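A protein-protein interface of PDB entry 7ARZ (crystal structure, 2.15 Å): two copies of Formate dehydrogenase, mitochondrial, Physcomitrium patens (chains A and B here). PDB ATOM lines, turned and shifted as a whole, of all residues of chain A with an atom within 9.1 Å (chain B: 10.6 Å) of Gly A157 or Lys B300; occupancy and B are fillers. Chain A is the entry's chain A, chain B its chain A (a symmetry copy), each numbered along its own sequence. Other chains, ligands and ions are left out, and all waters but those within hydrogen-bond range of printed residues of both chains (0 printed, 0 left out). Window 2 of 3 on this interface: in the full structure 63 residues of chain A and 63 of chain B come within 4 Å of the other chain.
Gly A150 touches Thr B313 (O to CA, 3.8 Å).
Trp A151 touches Thr B313 (N to CG2, 3.7 Å).
OE1 of Gln A153 touches CG of Pro B314, at 2.9 Å.
CG1 of Val A154 touches C of Thr B313 (3.6 Å).
Ser A155 touches Arg B305 (CA to O, 3.3 Å).
Ser A155 touches Tyr B306 (O to CE1, 3.3 Å).
CZ3 of Trp A159 touches NE1 of Trp B293, 3.5 Å away.
CH2 of Trp A159 touches CG of Gln B296, at 3.6 Å.
CE3 of Trp A159 touches N of Ala B298 (3.7 Å).
Pro B314 touches Trp A159.
Of chain B, only Lys B300, Arg B305 and Tyr B306 come within 4 Å of Gly A157.
Lys B300 touches one residue of chain A.
Of chain B, only Arg B305 (2.8 Å) comes within 4 Å of Gly A158.
No residue of chain A comes within 4 Å of Gly B299.
No residue of chain A comes within 4 Å of Asp B301.
Of the printed residues of chain A, Pro B314 touches Gly A150, Gln A153, Val A154 and Trp A159.
Of the printed residues of chain A, Pro B297 touches Trp A159.
Printed residues of chain B within 4 Å of Val A154: Arg B305 (2.9 Å), Met B312 (3.4 Å), Thr B313 (3.6 Å) and Pro B314 (3.4 Å).
The nearest residue of chain B that does not touch Gly A157 is Ala B298 (5.7 Å).
The nearest printed residue of chain A that does not touch Pro B297 is Asn A160 (7.2 Å).
The side-chain amide oxygen of Gln A153 is in hydrogen-bond range of the backbone NH of Asn A160, at 2.8 Å.
The backbone carbonyl oxygen (O) of Ala B298 sits at hydrogen-bond distance from the guanidinium group (NH2) of Arg B305 (2.9 Å).
The backbone carbonyl oxygen of Lys B300 sits close to the guanidinium group of Arg B305 (3.4 Å).
The side-chain hydroxyl of Tyr B306 is in hydrogen-bond range of the backbone carbonyl oxygen of Lys B300 (2.5 Å).
A ring nitrogen (NE2) of His B310 is in hydrogen-bond range of the backbone carbonyl oxygen of Arg B305, at 2.9 Å.
N of Met B312 lies within hydrogen-bond range of ND1 of His B310, at 2.9 Å.
Printed residues of chain B that touch a printed residue of chain A: Trp B293, Gln B296, Pro B297, Ala B298, Lys B300, Arg B305, Tyr B306, His B310, Met B312, Thr B313 and Pro B314.
Hydrophobic or aromatic side chains of chain B that line the printed part of chain A: Trp B293, Pro B297, Ala B298, Tyr B306, His B310, Met B312 and Pro B314.
Hydrophobic or aromatic side chains of chain A that line the printed part of chain B: Trp A151, Val A154 and Trp A159.
Among the printed residues, 22 pairs touch across the chains.
NE1 of Trp A151 is in hydrogen-bond range of O of His B310 (2.9 Å).
The backbone carbonyl oxygen (O) of Val A154 sits at hydrogen-bond distance from the guanidinium group (NH1) of Arg B305 (2.9 Å).
A ring nitrogen (NE2) of His B310 lies within hydrogen-bond range of the side-chain hydroxyl (OG) of Ser A155 (3.1 Å).
NH1 of Arg B305 sits close to O of Gly A157, at 3.3 Å.
O of Gly A158 sits at hydrogen-bond distance from NH1 of Arg B305, 2.8 Å away.
No position is printed for both chains.
Of the 22 pairs that touch across the chains among the printed residues, none has its exchanged pair printed and touching as well.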
ATOM      1  N   GLY A 150      12.096   8.588 -20.524  1.00  0.00           N
ATOM      2  CA  GLY A 150      11.007   9.258 -19.799  1.00  0.00           C
ATOM      3  C   GLY A 150      11.431  10.622 -19.276  1.00  0.00           C
ATOM      4  O   GLY A 150      10.655  11.569 -19.409  1.00  0.00           O
ATOM      5  N   TRP A 151      12.619  10.735 -18.681  1.00  0.00           N
ATOM      6  CA  TRP A 151      13.129  12.041 -18.196  1.00  0.00           C
ATOM      7  C   TRP A 151      13.315  12.968 -19.410  1.00  0.00           C
ATOM      8  O   TRP A 151      12.834  14.143 -19.369  1.00  0.00           O
ATOM      9  CB  TRP A 151      14.408  11.844 -17.386  1.00  0.00           C
ATOM     10  CG  TRP A 151      15.024  13.137 -16.948  1.00  0.00           C
ATOM     11  CD1 TRP A 151      14.620  13.928 -15.918  1.00  0.00           C
ATOM     12  CD2 TRP A 151      16.142  13.806 -17.553  1.00  0.00           C
ATOM     13  NE1 TRP A 151      15.412  15.045 -15.835  1.00  0.00           N
ATOM     14  CE2 TRP A 151      16.354  14.998 -16.824  1.00  0.00           C
ATOM     15  CE3 TRP A 151      16.989  13.516 -18.629  1.00  0.00           C
ATOM     16  CZ2 TRP A 151      17.385  15.884 -17.123  1.00  0.00           C
ATOM     17  CZ3 TRP A 151      18.020  14.383 -18.915  1.00  0.00           C
ATOM     18  CH2 TRP A 151      18.214  15.543 -18.166  1.00  0.00           C
ATOM     19  N   LYS A 152      13.914  12.454 -20.483  1.00  0.00           N
ATOM     20  CA  LYS A 152      14.101  13.221 -21.738  1.00  0.00           C
ATOM     21  C   LYS A 152      12.731  13.674 -22.233  1.00  0.00           C
ATOM     22  O   LYS A 152      12.579  14.858 -22.562  1.00  0.00           O
ATOM     23  CB  LYS A 152      14.820  12.360 -22.780  1.00  0.00           C
ATOM     24  CG  LYS A 152      15.055  13.010 -24.139  1.00  0.00           C
ATOM     25  CD  LYS A 152      15.847  12.103 -25.053  1.00  0.00           C
ATOM     26  CE  LYS A 152      15.788  12.478 -26.515  1.00  0.00           C
ATOM     27  NZ  LYS A 152      16.672  13.625 -26.809  1.00  0.00           N
ATOM     28  N   GLN A 153      11.761  12.753 -22.255  1.00  0.00           N
ATOM     29  CA  GLN A 153      10.444  13.000 -22.888  1.00  0.00           C
ATOM     30  C   GLN A 153       9.798  14.198 -22.199  1.00  0.00           C
ATOM     31  O   GLN A 153       9.345  15.089 -22.895  1.00  0.00           O
ATOM     32  CB  GLN A 153       9.569  11.735 -22.836  1.00  0.00           C
ATOM     33  CG  GLN A 153       8.181  11.910 -23.455  1.00  0.00           C
ATOM     34  CD  GLN A 153       7.233  10.796 -23.074  1.00  0.00           C
ATOM     35  OE1 GLN A 153       6.358  10.942 -22.212  1.00  0.00           O
ATOM     36  NE2 GLN A 153       7.454   9.648 -23.686  1.00  0.00           N
ATOM     37  N   VAL A 154       9.707  14.196 -20.874  1.00  0.00           N
ATOM     38  CA  VAL A 154       8.892  15.215 -20.153  1.00  0.00           C
ATOM     39  C   VAL A 154       9.648  16.545 -20.113  1.00  0.00           C
ATOM     40  O   VAL A 154       8.984  17.572 -19.997  1.00  0.00           O
ATOM     41  CB  VAL A 154       8.477  14.752 -18.744  1.00  0.00           C
ATOM     42  CG1 VAL A 154       7.507  13.584 -18.835  1.00  0.00           C
ATOM     43  CG2 VAL A 154       9.666  14.420 -17.841  1.00  0.00           C
ATOM     44  N   SER A 155      10.977  16.510 -20.221  1.00  0.00           N
ATOM     45  CA  SER A 155      11.852  17.714 -20.211  1.00  0.00           C
ATOM     46  C   SER A 155      11.687  18.476 -21.522  1.00  0.00           C
ATOM     47  O   SER A 155      11.898  19.676 -21.500  1.00  0.00           O
ATOM     48  CB  SER A 155      13.296  17.367 -19.957  1.00  0.00           C
ATOM     49  OG  SER A 155      13.429  16.844 -18.648  1.00  0.00           O
ATOM     50  N   GLU A 156      11.297  17.779 -22.592  1.00  0.00           N
ATOM     51  CA  GLU A 156      11.042  18.345 -23.938  1.00  0.00           C
ATOM     52  C   GLU A 156       9.531  18.515 -24.187  1.00  0.00           C
ATOM     53  O   GLU A 156       9.162  18.704 -25.341  1.00  0.00           O
ATOM     54  CB  GLU A 156      11.628  17.411 -24.998  1.00  0.00           C
ATOM     55  CG  GLU A 156      13.134  17.292 -24.969  1.00  0.00           C
ATOM     56  CD  GLU A 156      13.669  16.225 -25.914  1.00  0.00           C
ATOM     57  OE1 GLU A 156      12.847  15.598 -26.621  1.00  0.00           O
ATOM     58  OE2 GLU A 156      14.902  16.008 -25.937  1.00  0.00           O
ATOM     59  N   GLY A 157       8.674  18.366 -23.180  1.00  0.00           N
ATOM     60  CA  GLY A 157       7.246  18.747 -23.265  1.00  0.00           C
ATOM     61  C   GLY A 157       6.292  17.618 -23.662  1.00  0.00           C
ATOM     62  O   GLY A 157       5.079  17.873 -23.748  1.00  0.00           O
ATOM     63  N   GLY A 158       6.786  16.412 -23.916  1.00  0.00           N
ATOM     64  CA  GLY A 158       5.963  15.286 -24.413  1.00  0.00           C
ATOM     65  C   GLY A 158       5.184  14.600 -23.298  1.00  0.00           C
ATOM     66  O   GLY A 158       5.401  14.927 -22.115  1.00  0.00           O
ATOM     67  N   TRP A 159       4.264  13.699 -23.643  1.00  0.00           N
ATOM     68  CA  TRP A 159       3.620  12.790 -22.659  1.00  0.00           C
ATOM     69  C   TRP A 159       3.119  11.539 -23.375  1.00  0.00           C
ATOM     70  O   TRP A 159       2.097  11.608 -24.057  1.00  0.00           O
ATOM     71  CB  TRP A 159       2.501  13.475 -21.880  1.00  0.00           C
ATOM     72  CG  TRP A 159       1.861  12.554 -20.899  1.00  0.00           C
ATOM     73  CD1 TRP A 159       1.002  11.528 -21.179  1.00  0.00           C
ATOM     74  CD2 TRP A 159       2.046  12.539 -19.474  1.00  0.00           C
ATOM     75  NE1 TRP A 159       0.620  10.901 -20.025  1.00  0.00           N
ATOM     76  CE2 TRP A 159       1.247  11.492 -18.965  1.00  0.00           C
ATOM     77  CE3 TRP A 159       2.803  13.300 -18.586  1.00  0.00           C
ATOM     78  CZ2 TRP A 159       1.187  11.191 -17.604  1.00  0.00           C
ATOM     79  CZ3 TRP A 159       2.719  13.031 -17.239  1.00  0.00           C
ATOM     80  CH2 TRP A 159       1.942  11.974 -16.760  1.00  0.00           C
ATOM     81  N   ASN A 160       3.821  10.433 -23.164  1.00  0.00           N
ATOM     82  CA  ASN A 160       3.558   9.132 -23.807  1.00  0.00           C
ATOM     83  C   ASN A 160       4.086   8.052 -22.867  1.00  0.00           C
ATOM     84  O   ASN A 160       5.284   7.731 -22.912  1.00  0.00           O
ATOM     85  CB  ASN A 160       4.135   9.110 -25.222  1.00  0.00           C
ATOM     86  CG  ASN A 160       3.670   7.905 -25.999  1.00  0.00           C
ATOM     87  OD1 ASN A 160       3.122   6.976 -25.416  1.00  0.00           O
ATOM     88  ND2 ASN A 160       3.898   7.910 -27.299  1.00  0.00           N
ATOM     89  N   ASP B  59     -10.914  13.343 -21.843  1.00  0.00           N
ATOM     90  CA  ASP B  59     -10.646  14.762 -21.462  1.00  0.00           C
ATOM     91  C   ASP B  59     -11.607  15.670 -22.236  1.00  0.00           C
ATOM     92  O   ASP B  59     -11.797  15.439 -23.468  1.00  0.00           O
ATOM     93  CB  ASP B  59      -9.162  15.132 -21.664  1.00  0.00           C
ATOM     94  CG  ASP B  59      -8.251  14.873 -20.459  1.00  0.00           C
ATOM     95  OD1 ASP B  59      -8.771  14.617 -19.339  1.00  0.00           O
ATOM     96  OD2 ASP B  59      -7.011  14.938 -20.639  1.00  0.00           O
ATOM     97  N   TRP B 293       1.988  13.535 -11.378  1.00  0.00           N
ATOM     98  CA  TRP B 293       1.624  14.940 -11.673  1.00  0.00           C
ATOM     99  C   TRP B 293       0.195  15.214 -11.197  1.00  0.00           C
ATOM    100  O   TRP B 293      -0.625  14.247 -11.153  1.00  0.00           O
ATOM    101  CB  TRP B 293       1.769  15.203 -13.165  1.00  0.00           C
ATOM    102  CG  TRP B 293       3.075  14.737 -13.715  1.00  0.00           C
ATOM    103  CD1 TRP B 293       3.503  13.447 -13.798  1.00  0.00           C
ATOM    104  CD2 TRP B 293       4.138  15.551 -14.245  1.00  0.00           C
ATOM    105  NE1 TRP B 293       4.743  13.399 -14.363  1.00  0.00           N
ATOM    106  CE2 TRP B 293       5.167  14.667 -14.647  1.00  0.00           C
ATOM    107  CE3 TRP B 293       4.322  16.931 -14.432  1.00  0.00           C
ATOM    108  CZ2 TRP B 293       6.364  15.113 -15.215  1.00  0.00           C
ATOM    109  CZ3 TRP B 293       5.489  17.367 -15.027  1.00  0.00           C
ATOM    110  CH2 TRP B 293       6.504  16.475 -15.390  1.00  0.00           C
ATOM    111  N   ASN B 294      -0.091  16.481 -10.882  1.00  0.00           N
ATOM    112  CA  ASN B 294      -1.406  16.931 -10.358  1.00  0.00           C
ATOM    113  C   ASN B 294      -2.434  16.978 -11.497  1.00  0.00           C
ATOM    114  O   ASN B 294      -3.629  17.127 -11.223  1.00  0.00           O
ATOM    115  CB  ASN B 294      -1.280  18.282  -9.645  1.00  0.00           C
ATOM    116  CG  ASN B 294      -0.950  19.441 -10.558  1.00  0.00           C
ATOM    117  OD1 ASN B 294      -0.389  19.278 -11.647  1.00  0.00           O
ATOM    118  ND2 ASN B 294      -1.284  20.634 -10.093  1.00  0.00           N
ATOM    119  N   ALA B 295      -1.972  16.872 -12.728  1.00  0.00           N
ATOM    120  CA  ALA B 295      -2.800  16.736 -13.936  1.00  0.00           C
ATOM    121  C   ALA B 295      -2.148  15.663 -14.802  1.00  0.00           C
ATOM    122  O   ALA B 295      -0.943  15.764 -14.982  1.00  0.00           O
ATOM    123  CB  ALA B 295      -2.858  18.055 -14.657  1.00  0.00           C
ATOM    124  N   GLN B 296      -2.966  14.705 -15.272  1.00  0.00           N
ATOM    125  CA  GLN B 296      -2.576  13.514 -16.077  1.00  0.00           C
ATOM    126  C   GLN B 296      -3.505  13.249 -17.281  1.00  0.00           C
ATOM    127  O   GLN B 296      -4.660  12.963 -17.146  1.00  0.00           O
ATOM    128  CB  GLN B 296      -2.249  12.321 -15.178  1.00  0.00           C
ATOM    129  CG  GLN B 296      -0.885  12.421 -14.517  1.00  0.00           C
ATOM    130  CD  GLN B 296      -0.480  11.215 -13.710  1.00  0.00           C
ATOM    131  OE1 GLN B 296       0.178  11.321 -12.694  1.00  0.00           O
ATOM    132  NE2 GLN B 296      -0.878  10.051 -14.160  1.00  0.00           N
ATOM    133  N   PRO B 297      -2.819  13.491 -18.583  1.00  0.00           N
ATOM    134  CA  PRO B 297      -1.514  14.087 -18.888  1.00  0.00           C
ATOM    135  C   PRO B 297      -1.194  15.435 -18.208  1.00  0.00           C
ATOM    136  O   PRO B 297      -2.080  16.223 -17.965  1.00  0.00           O
ATOM    137  CB  PRO B 297      -1.596  14.305 -20.407  1.00  0.00           C
ATOM    138  CG  PRO B 297      -2.518  13.209 -20.894  1.00  0.00           C
ATOM    139  CD  PRO B 297      -3.550  13.092 -19.791  1.00  0.00           C
ATOM    140  N   ALA B 298       0.083  15.661 -17.903  1.00  0.00           N
ATOM    141  CA  ALA B 298       0.625  16.972 -17.485  1.00  0.00           C
ATOM    142  C   ALA B 298       0.596  17.902 -18.698  1.00  0.00           C
ATOM    143  O   ALA B 298       1.029  17.460 -19.779  1.00  0.00           O
ATOM    144  CB  ALA B 298       2.023  16.820 -16.931  1.00  0.00           C
ATOM    145  N   GLY B 299       0.043  19.109 -18.537  1.00  0.00           N
ATOM    146  CA  GLY B 299       0.094  20.166 -19.568  1.00  0.00           C
ATOM    147  C   GLY B 299       1.529  20.407 -20.001  1.00  0.00           C
ATOM    148  O   GLY B 299       2.439  20.214 -19.152  1.00  0.00           O
ATOM    149  N   LYS B 300       1.722  20.772 -21.272  1.00  0.00           N
ATOM    150  CA  LYS B 300       3.038  21.041 -21.926  1.00  0.00           C
ATOM    151  C   LYS B 300       3.891  21.999 -21.065  1.00  0.00           C
ATOM    152  O   LYS B 300       5.118  21.890 -21.102  1.00  0.00           O
ATOM    153  CB  LYS B 300       2.770  21.606 -23.324  1.00  0.00           C
ATOM    154  CG  LYS B 300       3.654  21.037 -24.426  1.00  0.00           C
ATOM    155  CD  LYS B 300       4.183  22.093 -25.407  1.00  0.00           C
ATOM    156  CE  LYS B 300       5.649  21.926 -25.780  1.00  0.00           C
ATOM    157  NZ  LYS B 300       5.869  20.827 -26.753  1.00  0.00           N
ATOM    158  N   ASP B 301       3.253  22.886 -20.299  1.00  0.00           N
ATOM    159  CA  ASP B 301       3.874  24.018 -19.572  1.00  0.00           C
ATOM    160  C   ASP B 301       3.904  23.701 -18.079  1.00  0.00           C
ATOM    161  O   ASP B 301       4.054  24.635 -17.285  1.00  0.00           O
ATOM    162  CB  ASP B 301       3.080  25.310 -19.805  1.00  0.00           C
ATOM    163  CG  ASP B 301       2.902  25.700 -21.268  1.00  0.00           C
ATOM    164  OD1 ASP B 301       3.871  25.559 -22.045  1.00  0.00           O
ATOM    165  OD2 ASP B 301       1.794  26.149 -21.615  1.00  0.00           O
ATOM    166  N   HIS B 302       3.748  22.438 -17.679  1.00  0.00           N
ATOM    167  CA  HIS B 302       3.896  22.067 -16.246  1.00  0.00           C
ATOM    168  C   HIS B 302       5.328  22.424 -15.854  1.00  0.00           C
ATOM    169  O   HIS B 302       6.278  22.023 -16.517  1.00  0.00           O
ATOM    170  CB  HIS B 302       3.551  20.598 -15.991  1.00  0.00           C
ATOM    171  CG  HIS B 302       3.286  20.324 -14.556  1.00  0.00           C
ATOM    172  ND1 HIS B 302       4.299  20.300 -13.615  1.00  0.00           N
ATOM    173  CD2 HIS B 302       2.132  20.082 -13.894  1.00  0.00           C
ATOM    174  CE1 HIS B 302       3.776  20.075 -12.422  1.00  0.00           C
ATOM    175  NE2 HIS B 302       2.435  19.899 -12.571  1.00  0.00           N
ATOM    176  N   PRO B 303       5.541  23.274 -14.834  1.00  0.00           N
ATOM    177  CA  PRO B 303       6.892  23.763 -14.555  1.00  0.00           C
ATOM    178  C   PRO B 303       7.845  22.634 -14.130  1.00  0.00           C
ATOM    179  O   PRO B 303       9.023  22.764 -14.331  1.00  0.00           O
ATOM    180  CB  PRO B 303       6.667  24.801 -13.444  1.00  0.00           C
ATOM    181  CG  PRO B 303       5.344  24.433 -12.808  1.00  0.00           C
ATOM    182  CD  PRO B 303       4.525  23.834 -13.931  1.00  0.00           C
ATOM    183  N   TRP B 304       7.318  21.552 -13.552  1.00  0.00           N
ATOM    184  CA  TRP B 304       8.141  20.431 -13.039  1.00  0.00           C
ATOM    185  C   TRP B 304       8.925  19.788 -14.175  1.00  0.00           C
ATOM    186  O   TRP B 304       9.919  19.107 -13.875  1.00  0.00           O
ATOM    187  CB  TRP B 304       7.280  19.404 -12.329  1.00  0.00           C
ATOM    188  CG  TRP B 304       6.812  19.871 -11.000  1.00  0.00           C
ATOM    189  CD1 TRP B 304       7.004  21.099 -10.457  1.00  0.00           C
ATOM    190  CD2 TRP B 304       6.027  19.126 -10.058  1.00  0.00           C
ATOM    191  NE1 TRP B 304       6.444  21.146  -9.213  1.00  0.00           N
ATOM    192  CE2 TRP B 304       5.813  19.969  -8.949  1.00  0.00           C
ATOM    193  CE3 TRP B 304       5.472  17.841 -10.048  1.00  0.00           C
ATOM    194  CZ2 TRP B 304       5.073  19.573  -7.834  1.00  0.00           C
ATOM    195  CZ3 TRP B 304       4.772  17.438  -8.934  1.00  0.00           C
ATOM    196  CH2 TRP B 304       4.565  18.293  -7.849  1.00  0.00           C
ATOM    197  N   ARG B 305       8.533  20.045 -15.416  1.00  0.00           N
ATOM    198  CA  ARG B 305       9.259  19.536 -16.605  1.00  0.00           C
ATOM    199  C   ARG B 305      10.567  20.291 -16.860  1.00  0.00           C
ATOM    200  O   ARG B 305      11.403  19.731 -17.584  1.00  0.00           O
ATOM    201  CB  ARG B 305       8.456  19.757 -17.883  1.00  0.00           C
ATOM    202  CG  ARG B 305       7.050  19.192 -17.879  1.00  0.00           C
ATOM    203  CD  ARG B 305       6.368  19.640 -19.158  1.00  0.00           C
ATOM    204  NE  ARG B 305       5.138  18.911 -19.435  1.00  0.00           N
ATOM    205  CZ  ARG B 305       5.059  17.804 -20.177  1.00  0.00           C
ATOM    206  NH1 ARG B 305       6.142  17.260 -20.717  1.00  0.00           N
ATOM    207  NH2 ARG B 305       3.879  17.242 -20.373  1.00  0.00           N
ATOM    208  N   TYR B 306      10.674  21.557 -16.439  1.00  0.00           N
ATOM    209  CA  TYR B 306      11.705  22.515 -16.941  1.00  0.00           C
ATOM    210  C   TYR B 306      12.521  23.115 -15.779  1.00  0.00           C
ATOM    211  O   TYR B 306      13.552  23.717 -16.034  1.00  0.00           O
ATOM    212  CB  TYR B 306      11.057  23.629 -17.774  1.00  0.00           C
ATOM    213  CG  TYR B 306      10.108  23.169 -18.849  1.00  0.00           C
ATOM    214  CD1 TYR B 306      10.568  22.524 -19.986  1.00  0.00           C
ATOM    215  CD2 TYR B 306       8.745  23.402 -18.742  1.00  0.00           C
ATOM    216  CE1 TYR B 306       9.700  22.105 -20.982  1.00  0.00           C
ATOM    217  CE2 TYR B 306       7.859  22.986 -19.724  1.00  0.00           C
ATOM    218  CZ  TYR B 306       8.338  22.345 -20.855  1.00  0.00           C
ATOM    219  OH  TYR B 306       7.471  21.941 -21.834  1.00  0.00           O
ATOM    220  N   MET B 307      12.079  22.936 -14.538  1.00  0.00           N
ATOM    221  CA  MET B 307      12.831  23.327 -13.320  1.00  0.00           C
ATOM    222  C   MET B 307      14.195  22.622 -13.252  1.00  0.00           C
ATOM    223  O   MET B 307      14.464  21.623 -13.918  1.00  0.00           O
ATOM    224  CB  MET B 307      12.002  23.045 -12.058  1.00  0.00           C
ATOM    225  CG  MET B 307      11.773  21.574 -11.723  1.00  0.00           C
ATOM    226  SD  MET B 307      10.525  21.445 -10.409  1.00  0.00           S
ATOM    227  CE  MET B 307      10.532  19.691 -10.040  1.00  0.00           C
ATOM    228  N   HIS B 310      15.700  18.159 -11.678  1.00  0.00           N
ATOM    229  CA  HIS B 310      14.479  17.309 -11.577  1.00  0.00           C
ATOM    230  C   HIS B 310      14.766  15.914 -12.136  1.00  0.00           C
ATOM    231  O   HIS B 310      15.603  15.769 -13.055  1.00  0.00           O
ATOM    232  CB  HIS B 310      13.242  17.968 -12.190  1.00  0.00           C
ATOM    233  CG  HIS B 310      13.079  17.747 -13.651  1.00  0.00           C
ATOM    234  ND1 HIS B 310      12.932  16.489 -14.196  1.00  0.00           N
ATOM    235  CD2 HIS B 310      12.974  18.625 -14.671  1.00  0.00           C
ATOM    236  CE1 HIS B 310      12.781  16.600 -15.502  1.00  0.00           C
ATOM    237  NE2 HIS B 310      12.796  17.900 -15.820  1.00  0.00           N
ATOM    238  N   MET B 312      12.012  13.944 -13.148  1.00  0.00           N
ATOM    239  CA  MET B 312      10.591  13.727 -13.544  1.00  0.00           C
ATOM    240  C   MET B 312      10.583  12.789 -14.749  1.00  0.00           C
ATOM    241  O   MET B 312      11.551  12.830 -15.519  1.00  0.00           O
ATOM    242  CB  MET B 312       9.863  15.025 -13.928  1.00  0.00           C
ATOM    243  CG  MET B 312       9.774  16.050 -12.812  1.00  0.00           C
ATOM    244  SD  MET B 312       9.142  15.394 -11.249  1.00  0.00           S
ATOM    245  CE  MET B 312       7.448  15.070 -11.751  1.00  0.00           C
ATOM    246  N   THR B 313       9.535  11.960 -14.842  1.00  0.00           N
ATOM    247  CA  THR B 313       9.134  11.119 -15.997  1.00  0.00           C
ATOM    248  C   THR B 313       7.617  11.200 -16.093  1.00  0.00           C
ATOM    249  O   THR B 313       6.981  11.651 -15.154  1.00  0.00           O
ATOM    250  CB  THR B 313       9.511   9.639 -15.800  1.00  0.00           C
ATOM    251  OG1 THR B 313       8.883   9.171 -14.603  1.00  0.00           O
ATOM    252  CG2 THR B 313      10.998   9.388 -15.690  1.00  0.00           C
ATOM    253  N   PRO B 314       6.959  10.664 -17.142  1.00  0.00           N
ATOM    254  CA  PRO B 314       5.518  10.455 -17.081  1.00  0.00           C
ATOM    255  C   PRO B 314       5.258   9.403 -16.003  1.00  0.00           C
ATOM    256  O   PRO B 314       6.212   8.892 -15.428  1.00  0.00           O
ATOM    257  CB  PRO B 314       5.160   9.955 -18.483  1.00  0.00           C
ATOM    258  CG  PRO B 314       6.344  10.309 -19.347  1.00  0.00           C
ATOM    259  CD  PRO B 314       7.534  10.223 -18.419  1.00  0.00           C
